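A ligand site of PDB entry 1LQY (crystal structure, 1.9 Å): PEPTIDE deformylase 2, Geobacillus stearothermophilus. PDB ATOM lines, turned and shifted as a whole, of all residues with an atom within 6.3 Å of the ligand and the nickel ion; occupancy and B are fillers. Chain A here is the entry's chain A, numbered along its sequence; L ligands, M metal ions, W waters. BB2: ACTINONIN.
The side-chain hydroxyl (OG1) of Thr 106 is in hydrogen-bond range of an oxygen (O27) of the ligand.
The side-chain carboxylate (OE2) of Glu 154 sits at hydrogen-bond distance from a nitrogen (N1) of the ligand.
An oxygen (O2) of the ligand lies close to the side-chain amide oxygen (OE1) of Gln 65, 2.7 Å away.
The backbone NH of Leu 111 lies close to an oxygen (O4) of the ligand, at 2.9 Å.
An oxygen (O20) of the ligand lies within hydrogen-bond range of the backbone NH (N) of Gly 109, 3.0 Å away.
N14 of the ligand is in hydrogen-bond range of O of Gly 109, at 3.0 Å.
The backbone carbonyl oxygen of Gly 60 sits at hydrogen-bond distance from a nitrogen (N1) of the ligand (3.0 Å).
N of Ile 59 is in hydrogen-bond range of O13 of the ligand, at 3.0 Å.
O of Gly 107 is in hydrogen-bond range of O27 of the ligand.
A ring nitrogen (ND1) of His 153 sits at hydrogen-bond distance from the side-chain carboxylate (OE1) of Glu 108, 3.1 Å away.
NE2 of His 157 sits close to NE2 of Gln 65 (3.5 Å).
N of Ala 62 is in hydrogen-bond range of OE1 of Glu 154, 3.5 Å away.
OE1 of Gln 65 is in hydrogen-bond range of N of Ala 62 (2.9 Å).
The side-chain sulfur (SG) of Cys 110 lies close to the backbone NH (N) of Ser 112, 3.7 Å away.
OE1 of Glu 108 is in salt-bridge range of NH2 of Arg 123, 2.8 Å away.
O of Pro 57 touches C17 of the ligand, 3.7 Å away.
CA of Gly 58 touches O13 of the ligand (3.2 Å).
Leu 104 touches the ligand.
CA of Glu 108 touches O20 of the ligand, 3.7 Å away.
Hydrophobic or aromatic side chains within 4 Å of the ligand: Ile 59, Leu 104, Leu 111, His 153 and His 157.
Within 4 Å of the ligand: Pro 57, Gly 58, Ile 59, Gly 60, Gln 65, Leu 104, Thr 106, Gly 107, Glu 108, Gly 109, Cys 110, Leu 111, His 153, Glu 154 and His 157.
Merely in contact with the nickel ion: Gln 65.
The nearest printed residue that does not touch the nickel ion is Glu 154 (4.4 Å).
The nickel ion is bound by a ring nitrogen (NE2) of His 153 (2.1 Å), an oxygen (O2) of the ligand (2.1 Å), a ring nitrogen (NE2) of His 157 (2.2 Å), an oxygen (O4) of the ligand (2.2 Å) and the side-chain sulfur of Cys 110 (2.7 Å).
The nickel ion has five donor atoms within binding distance.
Water W3 bridges O of Pro 57 and O13 of the ligand.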
ATOM      1  N   PRO A  57       8.282 -10.267 -17.145  1.00  0.00           N
ATOM      2  CA  PRO A  57       7.020 -10.767 -17.694  1.00  0.00           C
ATOM      3  C   PRO A  57       6.223 -11.709 -16.802  1.00  0.00           C
ATOM      4  O   PRO A  57       6.733 -12.720 -16.305  1.00  0.00           O
ATOM      5  CB  PRO A  57       7.422 -11.418 -19.035  1.00  0.00           C
ATOM      6  CG  PRO A  57       8.880 -11.603 -18.979  1.00  0.00           C
ATOM      7  CD  PRO A  57       9.446 -10.634 -17.970  1.00  0.00           C
ATOM      8  N   GLY A  58       4.966 -11.350 -16.597  1.00  0.00           N
ATOM      9  CA  GLY A  58       4.084 -12.186 -15.807  1.00  0.00           C
ATOM     10  C   GLY A  58       2.754 -12.257 -16.532  1.00  0.00           C
ATOM     11  O   GLY A  58       2.313 -11.258 -17.123  1.00  0.00           O
ATOM     12  N   ILE A  59       2.101 -13.420 -16.509  1.00  0.00           N
ATOM     13  CA  ILE A  59       0.812 -13.538 -17.156  1.00  0.00           C
ATOM     14  C   ILE A  59      -0.323 -13.410 -16.131  1.00  0.00           C
ATOM     15  O   ILE A  59      -1.502 -13.561 -16.450  1.00  0.00           O
ATOM     16  CB  ILE A  59       0.703 -14.872 -17.920  1.00  0.00           C
ATOM     17  CG1 ILE A  59       1.035 -16.054 -17.009  1.00  0.00           C
ATOM     18  CG2 ILE A  59       1.680 -14.861 -19.062  1.00  0.00           C
ATOM     19  CD1 ILE A  59       0.908 -17.406 -17.719  1.00  0.00           C
ATOM     20  N   GLY A  60       0.069 -13.131 -14.888  1.00  0.00           N
ATOM     21  CA  GLY A  60      -0.918 -12.914 -13.831  1.00  0.00           C
ATOM     22  C   GLY A  60      -0.259 -12.205 -12.656  1.00  0.00           C
ATOM     23  O   GLY A  60       0.960 -12.241 -12.507  1.00  0.00           O
ATOM     24  N   LEU A  61      -1.035 -11.526 -11.813  1.00  0.00           N
ATOM     25  CA  LEU A  61      -0.429 -10.886 -10.646  1.00  0.00           C
ATOM     26  C   LEU A  61      -1.461 -10.726  -9.517  1.00  0.00           C
ATOM     27  O   LEU A  61      -2.633 -10.518  -9.784  1.00  0.00           O
ATOM     28  CB  LEU A  61       0.136  -9.505 -11.010  1.00  0.00           C
ATOM     29  CG  LEU A  61       0.992  -8.885  -9.900  1.00  0.00           C
ATOM     30  CD1 LEU A  61       2.342  -9.560  -9.803  1.00  0.00           C
ATOM     31  CD2 LEU A  61       1.127  -7.399 -10.187  1.00  0.00           C
ATOM     32  N   ALA A  62      -0.999 -10.816  -8.265  1.00  0.00           N
ATOM     33  CA  ALA A  62      -1.934 -10.659  -7.118  1.00  0.00           C
ATOM     34  C   ALA A  62      -1.487  -9.517  -6.164  1.00  0.00           C
ATOM     35  O   ALA A  62      -0.307  -9.288  -5.989  1.00  0.00           O
ATOM     36  CB  ALA A  62      -2.049 -11.980  -6.370  1.00  0.00           C
ATOM     37  N   GLN A  65       1.620  -9.487  -3.858  1.00  0.00           N
ATOM     38  CA  GLN A  65       2.989  -9.467  -4.418  1.00  0.00           C
ATOM     39  C   GLN A  65       3.619  -8.064  -4.395  1.00  0.00           C
ATOM     40  O   GLN A  65       4.841  -7.938  -4.471  1.00  0.00           O
ATOM     41  CB  GLN A  65       3.028 -10.057  -5.839  1.00  0.00           C
ATOM     42  CG  GLN A  65       2.767 -11.552  -5.834  1.00  0.00           C
ATOM     43  CD  GLN A  65       2.621 -12.129  -7.216  1.00  0.00           C
ATOM     44  OE1 GLN A  65       1.590 -11.968  -7.884  1.00  0.00           O
ATOM     45  NE2 GLN A  65       3.667 -12.793  -7.664  1.00  0.00           N
ATOM     46  N   LEU A 104       1.835 -27.857 -15.950  1.00  0.00           N
ATOM     47  CA  LEU A 104       2.753 -27.440 -17.027  1.00  0.00           C
ATOM     48  C   LEU A 104       3.999 -28.329 -16.922  1.00  0.00           C
ATOM     49  O   LEU A 104       4.571 -28.486 -15.846  1.00  0.00           O
ATOM     50  CB  LEU A 104       3.167 -25.971 -16.802  1.00  0.00           C
ATOM     51  CG  LEU A 104       2.456 -24.839 -17.533  1.00  0.00           C
ATOM     52  CD1 LEU A 104       1.091 -25.197 -17.954  1.00  0.00           C
ATOM     53  CD2 LEU A 104       2.440 -23.625 -16.631  1.00  0.00           C
ATOM     54  N   THR A 106       6.900 -27.717 -17.838  1.00  0.00           N
ATOM     55  CA  THR A 106       8.064 -26.885 -17.501  1.00  0.00           C
ATOM     56  C   THR A 106       8.084 -26.497 -16.028  1.00  0.00           C
ATOM     57  O   THR A 106       9.096 -25.978 -15.536  1.00  0.00           O
ATOM     58  CB  THR A 106       8.032 -25.532 -18.226  1.00  0.00           C
ATOM     59  OG1 THR A 106       6.848 -24.833 -17.834  1.00  0.00           O
ATOM     60  CG2 THR A 106       8.078 -25.709 -19.731  1.00  0.00           C
ATOM     61  N   GLY A 107       6.979 -26.734 -15.324  1.00  0.00           N
ATOM     62  CA  GLY A 107       6.896 -26.289 -13.938  1.00  0.00           C
ATOM     63  C   GLY A 107       6.447 -24.827 -14.030  1.00  0.00           C
ATOM     64  O   GLY A 107       6.136 -24.338 -15.131  1.00  0.00           O
ATOM     65  N   GLU A 108       6.371 -24.139 -12.898  1.00  0.00           N
ATOM     66  CA  GLU A 108       5.930 -22.762 -12.880  1.00  0.00           C
ATOM     67  C   GLU A 108       7.018 -21.854 -12.269  1.00  0.00           C
ATOM     68  O   GLU A 108       7.879 -22.300 -11.483  1.00  0.00           O
ATOM     69  CB  GLU A 108       4.631 -22.603 -12.052  1.00  0.00           C
ATOM     70  CG  GLU A 108       3.436 -23.413 -12.577  1.00  0.00           C
ATOM     71  CD  GLU A 108       2.171 -23.264 -11.728  1.00  0.00           C
ATOM     72  OE1 GLU A 108       2.141 -22.416 -10.782  1.00  0.00           O
ATOM     73  OE2 GLU A 108       1.182 -23.983 -12.014  1.00  0.00           O
ATOM     74  N   GLY A 109       6.957 -20.583 -12.639  1.00  0.00           N
ATOM     75  CA  GLY A 109       7.881 -19.617 -12.079  1.00  0.00           C
ATOM     76  C   GLY A 109       7.007 -18.589 -11.371  1.00  0.00           C
ATOM     77  O   GLY A 109       5.820 -18.458 -11.691  1.00  0.00           O
ATOM     78  N   CYS A 110       7.597 -17.867 -10.417  1.00  0.00           N
ATOM     79  CA  CYS A 110       6.858 -16.862  -9.662  1.00  0.00           C
ATOM     80  C   CYS A 110       7.689 -15.583  -9.611  1.00  0.00           C
ATOM     81  O   CYS A 110       8.894 -15.624  -9.405  1.00  0.00           O
ATOM     82  CB  CYS A 110       6.587 -17.351  -8.203  1.00  0.00           C
ATOM     83  SG  CYS A 110       5.422 -16.320  -7.241  1.00  0.00           S
ATOM     84  N   LEU A 111       7.035 -14.462  -9.799  1.00  0.00           N
ATOM     85  CA  LEU A 111       7.760 -13.182  -9.775  1.00  0.00           C
ATOM     86  C   LEU A 111       8.433 -12.958  -8.417  1.00  0.00           C
ATOM     87  O   LEU A 111       9.464 -12.311  -8.344  1.00  0.00           O
ATOM     88  CB  LEU A 111       6.779 -12.051 -10.106  1.00  0.00           C
ATOM     89  CG  LEU A 111       6.784 -11.456 -11.512  1.00  0.00           C
ATOM     90  CD1 LEU A 111       7.085 -12.500 -12.539  1.00  0.00           C
ATOM     91  CD2 LEU A 111       5.446 -10.799 -11.804  1.00  0.00           C
ATOM     92  N   SER A 112       7.852 -13.497  -7.324  1.00  0.00           N
ATOM     93  CA  SER A 112       8.456 -13.318  -5.995  1.00  0.00           C
ATOM     94  C   SER A 112       9.535 -14.376  -5.646  1.00  0.00           C
ATOM     95  O   SER A 112      10.164 -14.293  -4.575  1.00  0.00           O
ATOM     96  CB  SER A 112       7.357 -13.339  -4.911  1.00  0.00           C
ATOM     97  OG  SER A 112       6.239 -12.530  -5.248  1.00  0.00           O
ATOM     98  N   ARG A 123      -2.467 -28.893 -10.637  1.00  0.00           N
ATOM     99  CA  ARG A 123      -3.579 -27.962 -10.672  1.00  0.00           C
ATOM    100  C   ARG A 123      -4.827 -28.662 -11.171  1.00  0.00           C
ATOM    101  O   ARG A 123      -4.743 -29.720 -11.798  1.00  0.00           O
ATOM    102  CB  ARG A 123      -3.267 -26.812 -11.639  1.00  0.00           C
ATOM    103  CG  ARG A 123      -1.929 -26.081 -11.385  1.00  0.00           C
ATOM    104  CD  ARG A 123      -2.170 -24.936 -10.416  1.00  0.00           C
ATOM    105  NE  ARG A 123      -1.025 -24.059 -10.155  1.00  0.00           N
ATOM    106  CZ  ARG A 123      -0.900 -23.334  -9.040  1.00  0.00           C
ATOM    107  NH1 ARG A 123      -1.844 -23.406  -8.107  1.00  0.00           N
ATOM    108  NH2 ARG A 123       0.159 -22.543  -8.839  1.00  0.00           N
ATOM    109  N   LEU A 146      -4.303 -23.615 -19.341  1.00  0.00           N
ATOM    110  CA  LEU A 146      -3.430 -22.546 -18.854  1.00  0.00           C
ATOM    111  C   LEU A 146      -4.204 -21.418 -18.189  1.00  0.00           C
ATOM    112  O   LEU A 146      -3.774 -20.916 -17.157  1.00  0.00           O
ATOM    113  CB  LEU A 146      -2.541 -21.996 -19.965  1.00  0.00           C
ATOM    114  CG  LEU A 146      -1.586 -20.883 -19.513  1.00  0.00           C
ATOM    115  CD1 LEU A 146      -0.585 -21.384 -18.471  1.00  0.00           C
ATOM    116  CD2 LEU A 146      -0.819 -20.395 -20.744  1.00  0.00           C
ATOM    117  N   ILE A 149      -5.024 -22.526 -14.738  1.00  0.00           N
ATOM    118  CA  ILE A 149      -3.816 -22.602 -13.943  1.00  0.00           C
ATOM    119  C   ILE A 149      -3.435 -21.215 -13.441  1.00  0.00           C
ATOM    120  O   ILE A 149      -3.100 -21.064 -12.261  1.00  0.00           O
ATOM    121  CB  ILE A 149      -2.648 -23.206 -14.792  1.00  0.00           C
ATOM    122  CG1 ILE A 149      -2.952 -24.687 -15.072  1.00  0.00           C
ATOM    123  CG2 ILE A 149      -1.347 -23.172 -14.010  1.00  0.00           C
ATOM    124  CD1 ILE A 149      -1.804 -25.413 -15.754  1.00  0.00           C
ATOM    125  N   VAL A 150      -3.469 -20.204 -14.324  1.00  0.00           N
ATOM    126  CA  VAL A 150      -3.099 -18.853 -13.895  1.00  0.00           C
ATOM    127  C   VAL A 150      -4.030 -18.351 -12.790  1.00  0.00           C
ATOM    128  O   VAL A 150      -3.566 -17.786 -11.796  1.00  0.00           O
ATOM    129  CB  VAL A 150      -3.116 -17.824 -15.092  1.00  0.00           C
ATOM    130  CG1 VAL A 150      -2.589 -16.486 -14.599  1.00  0.00           C
ATOM    131  CG2 VAL A 150      -2.216 -18.319 -16.256  1.00  0.00           C
ATOM    132  N   HIS A 153      -3.065 -20.024  -9.574  1.00  0.00           N
ATOM    133  CA  HIS A 153      -1.816 -19.475  -9.052  1.00  0.00           C
ATOM    134  C   HIS A 153      -2.047 -18.110  -8.344  1.00  0.00           C
ATOM    135  O   HIS A 153      -1.560 -17.892  -7.231  1.00  0.00           O
ATOM    136  CB  HIS A 153      -0.828 -19.276 -10.234  1.00  0.00           C
ATOM    137  CG  HIS A 153       0.506 -18.711  -9.815  1.00  0.00           C
ATOM    138  ND1 HIS A 153       1.668 -19.456  -9.857  1.00  0.00           N
ATOM    139  CD2 HIS A 153       0.860 -17.476  -9.395  1.00  0.00           C
ATOM    140  CE1 HIS A 153       2.680 -18.702  -9.470  1.00  0.00           C
ATOM    141  NE2 HIS A 153       2.215 -17.494  -9.181  1.00  0.00           N
ATOM    142  N   GLU A 154      -2.786 -17.217  -8.967  1.00  0.00           N
ATOM    143  CA  GLU A 154      -3.018 -15.894  -8.367  1.00  0.00           C
ATOM    144  C   GLU A 154      -3.960 -16.007  -7.166  1.00  0.00           C
ATOM    145  O   GLU A 154      -3.770 -15.352  -6.147  1.00  0.00           O
ATOM    146  CB  GLU A 154      -3.620 -14.889  -9.369  1.00  0.00           C
ATOM    147  CG  GLU A 154      -2.824 -14.666 -10.690  1.00  0.00           C
ATOM    148  CD  GLU A 154      -1.317 -14.572 -10.489  1.00  0.00           C
ATOM    149  OE1 GLU A 154      -0.845 -14.078  -9.424  1.00  0.00           O
ATOM    150  OE2 GLU A 154      -0.578 -14.993 -11.405  1.00  0.00           O
ATOM    151  N   HIS A 157      -2.072 -17.032  -4.074  1.00  0.00           N
ATOM    152  CA  HIS A 157      -1.369 -15.946  -3.382  1.00  0.00           C
ATOM    153  C   HIS A 157      -2.248 -15.268  -2.344  1.00  0.00           C
ATOM    154  O   HIS A 157      -1.729 -14.849  -1.307  1.00  0.00           O
ATOM    155  CB  HIS A 157      -0.908 -14.844  -4.334  1.00  0.00           C
ATOM    156  CG  HIS A 157       0.333 -15.172  -5.073  1.00  0.00           C
ATOM    157  ND1 HIS A 157       1.501 -15.545  -4.436  1.00  0.00           N
ATOM    158  CD2 HIS A 157       0.612 -15.180  -6.404  1.00  0.00           C
ATOM    159  CE1 HIS A 157       2.437 -15.767  -5.345  1.00  0.00           C
ATOM    160  NE2 HIS A 157       1.917 -15.555  -6.543  1.00  0.00           N
ATOM    161  N   PHE A 163       3.357 -21.558  -5.154  1.00  0.00           N
ATOM    162  CA  PHE A 163       3.298 -22.672  -6.102  1.00  0.00           C
ATOM    163  C   PHE A 163       4.039 -23.919  -5.665  1.00  0.00           C
ATOM    164  O   PHE A 163       3.537 -25.030  -5.839  1.00  0.00           O
ATOM    165  CB  PHE A 163       3.778 -22.203  -7.489  1.00  0.00           C
ATOM    166  CG  PHE A 163       5.285 -22.083  -7.608  1.00  0.00           C
ATOM    167  CD1 PHE A 163       6.059 -23.170  -8.021  1.00  0.00           C
ATOM    168  CD2 PHE A 163       5.921 -20.859  -7.371  1.00  0.00           C
ATOM    169  CE1 PHE A 163       7.455 -23.054  -8.217  1.00  0.00           C
ATOM    170  CE2 PHE A 163       7.313 -20.727  -7.568  1.00  0.00           C
ATOM    171  CZ  PHE A 163       8.073 -21.829  -7.994  1.00  0.00           C
HETATM  172  C5  BB2 L   1       3.675 -14.548 -12.477  1.00  0.00           C
HETATM  173  C3  BB2 L   1       3.316 -14.555 -10.965  1.00  0.00           C
HETATM  174  O4  BB2 L   1       4.165 -14.845 -10.114  1.00  0.00           O
HETATM  175  N1  BB2 L   1       2.077 -14.246 -10.601  1.00  0.00           N
HETATM  176  O2  BB2 L   1       1.741 -14.253  -9.232  1.00  0.00           O
HETATM  177  C6  BB2 L   1       3.470 -15.983 -12.975  1.00  0.00           C
HETATM  178  C12 BB2 L   1       4.220 -16.161 -14.328  1.00  0.00           C
HETATM  179  O13 BB2 L   1       4.004 -15.366 -15.280  1.00  0.00           O
HETATM  180  C7  BB2 L   1       1.930 -16.230 -13.154  1.00  0.00           C
HETATM  181  C8  BB2 L   1       1.529 -17.537 -13.892  1.00  0.00           C
HETATM  182  C9  BB2 L   1       1.900 -18.771 -13.081  1.00  0.00           C
HETATM  183  C10 BB2 L   1       1.128 -20.001 -13.627  1.00  0.00           C
HETATM  184  C11 BB2 L   1       1.691 -20.617 -14.916  1.00  0.00           C
HETATM  185  N14 BB2 L   1       5.071 -17.274 -14.327  1.00  0.00           N
HETATM  186  C15 BB2 L   1       5.768 -17.494 -15.541  1.00  0.00           C
HETATM  187  C16 BB2 L   1       7.305 -17.405 -15.335  1.00  0.00           C
HETATM  188  C18 BB2 L   1       8.093 -17.812 -16.613  1.00  0.00           C
HETATM  189  C17 BB2 L   1       7.704 -15.979 -14.917  1.00  0.00           C
HETATM  190  C19 BB2 L   1       5.406 -18.944 -15.990  1.00  0.00           C
HETATM  191  O20 BB2 L   1       5.462 -19.827 -15.097  1.00  0.00           O
HETATM  192  N21 BB2 L   1       5.219 -19.260 -17.317  1.00  0.00           N
HETATM  193  C22 BB2 L   1       4.638 -20.587 -17.664  1.00  0.00           C
HETATM  194  C23 BB2 L   1       4.505 -18.226 -18.097  1.00  0.00           C
HETATM  195  C24 BB2 L   1       4.021 -19.001 -19.345  1.00  0.00           C
HETATM  196  C25 BB2 L   1       3.574 -20.319 -18.734  1.00  0.00           C
HETATM  197  C26 BB2 L   1       5.869 -21.381 -18.106  1.00  0.00           C
HETATM  198  O27 BB2 L   1       5.785 -22.595 -18.124  1.00  0.00           O
HETATM  199 NI    NI M   1       3.060 -15.713  -8.377  1.00  0.00          NI
HETATM  200  O   HOH W   1       9.509 -13.179 -15.549  1.00  0.00           O
HETATM  201  O   HOH W   2       4.245 -23.954 -20.526  1.00  0.00           O
HETATM  202  O   HOH W   3       5.642 -14.694 -17.771  1.00  0.00           O
HETATM  203  O   HOH W   4      10.291 -18.628 -14.187  1.00  0.00           O
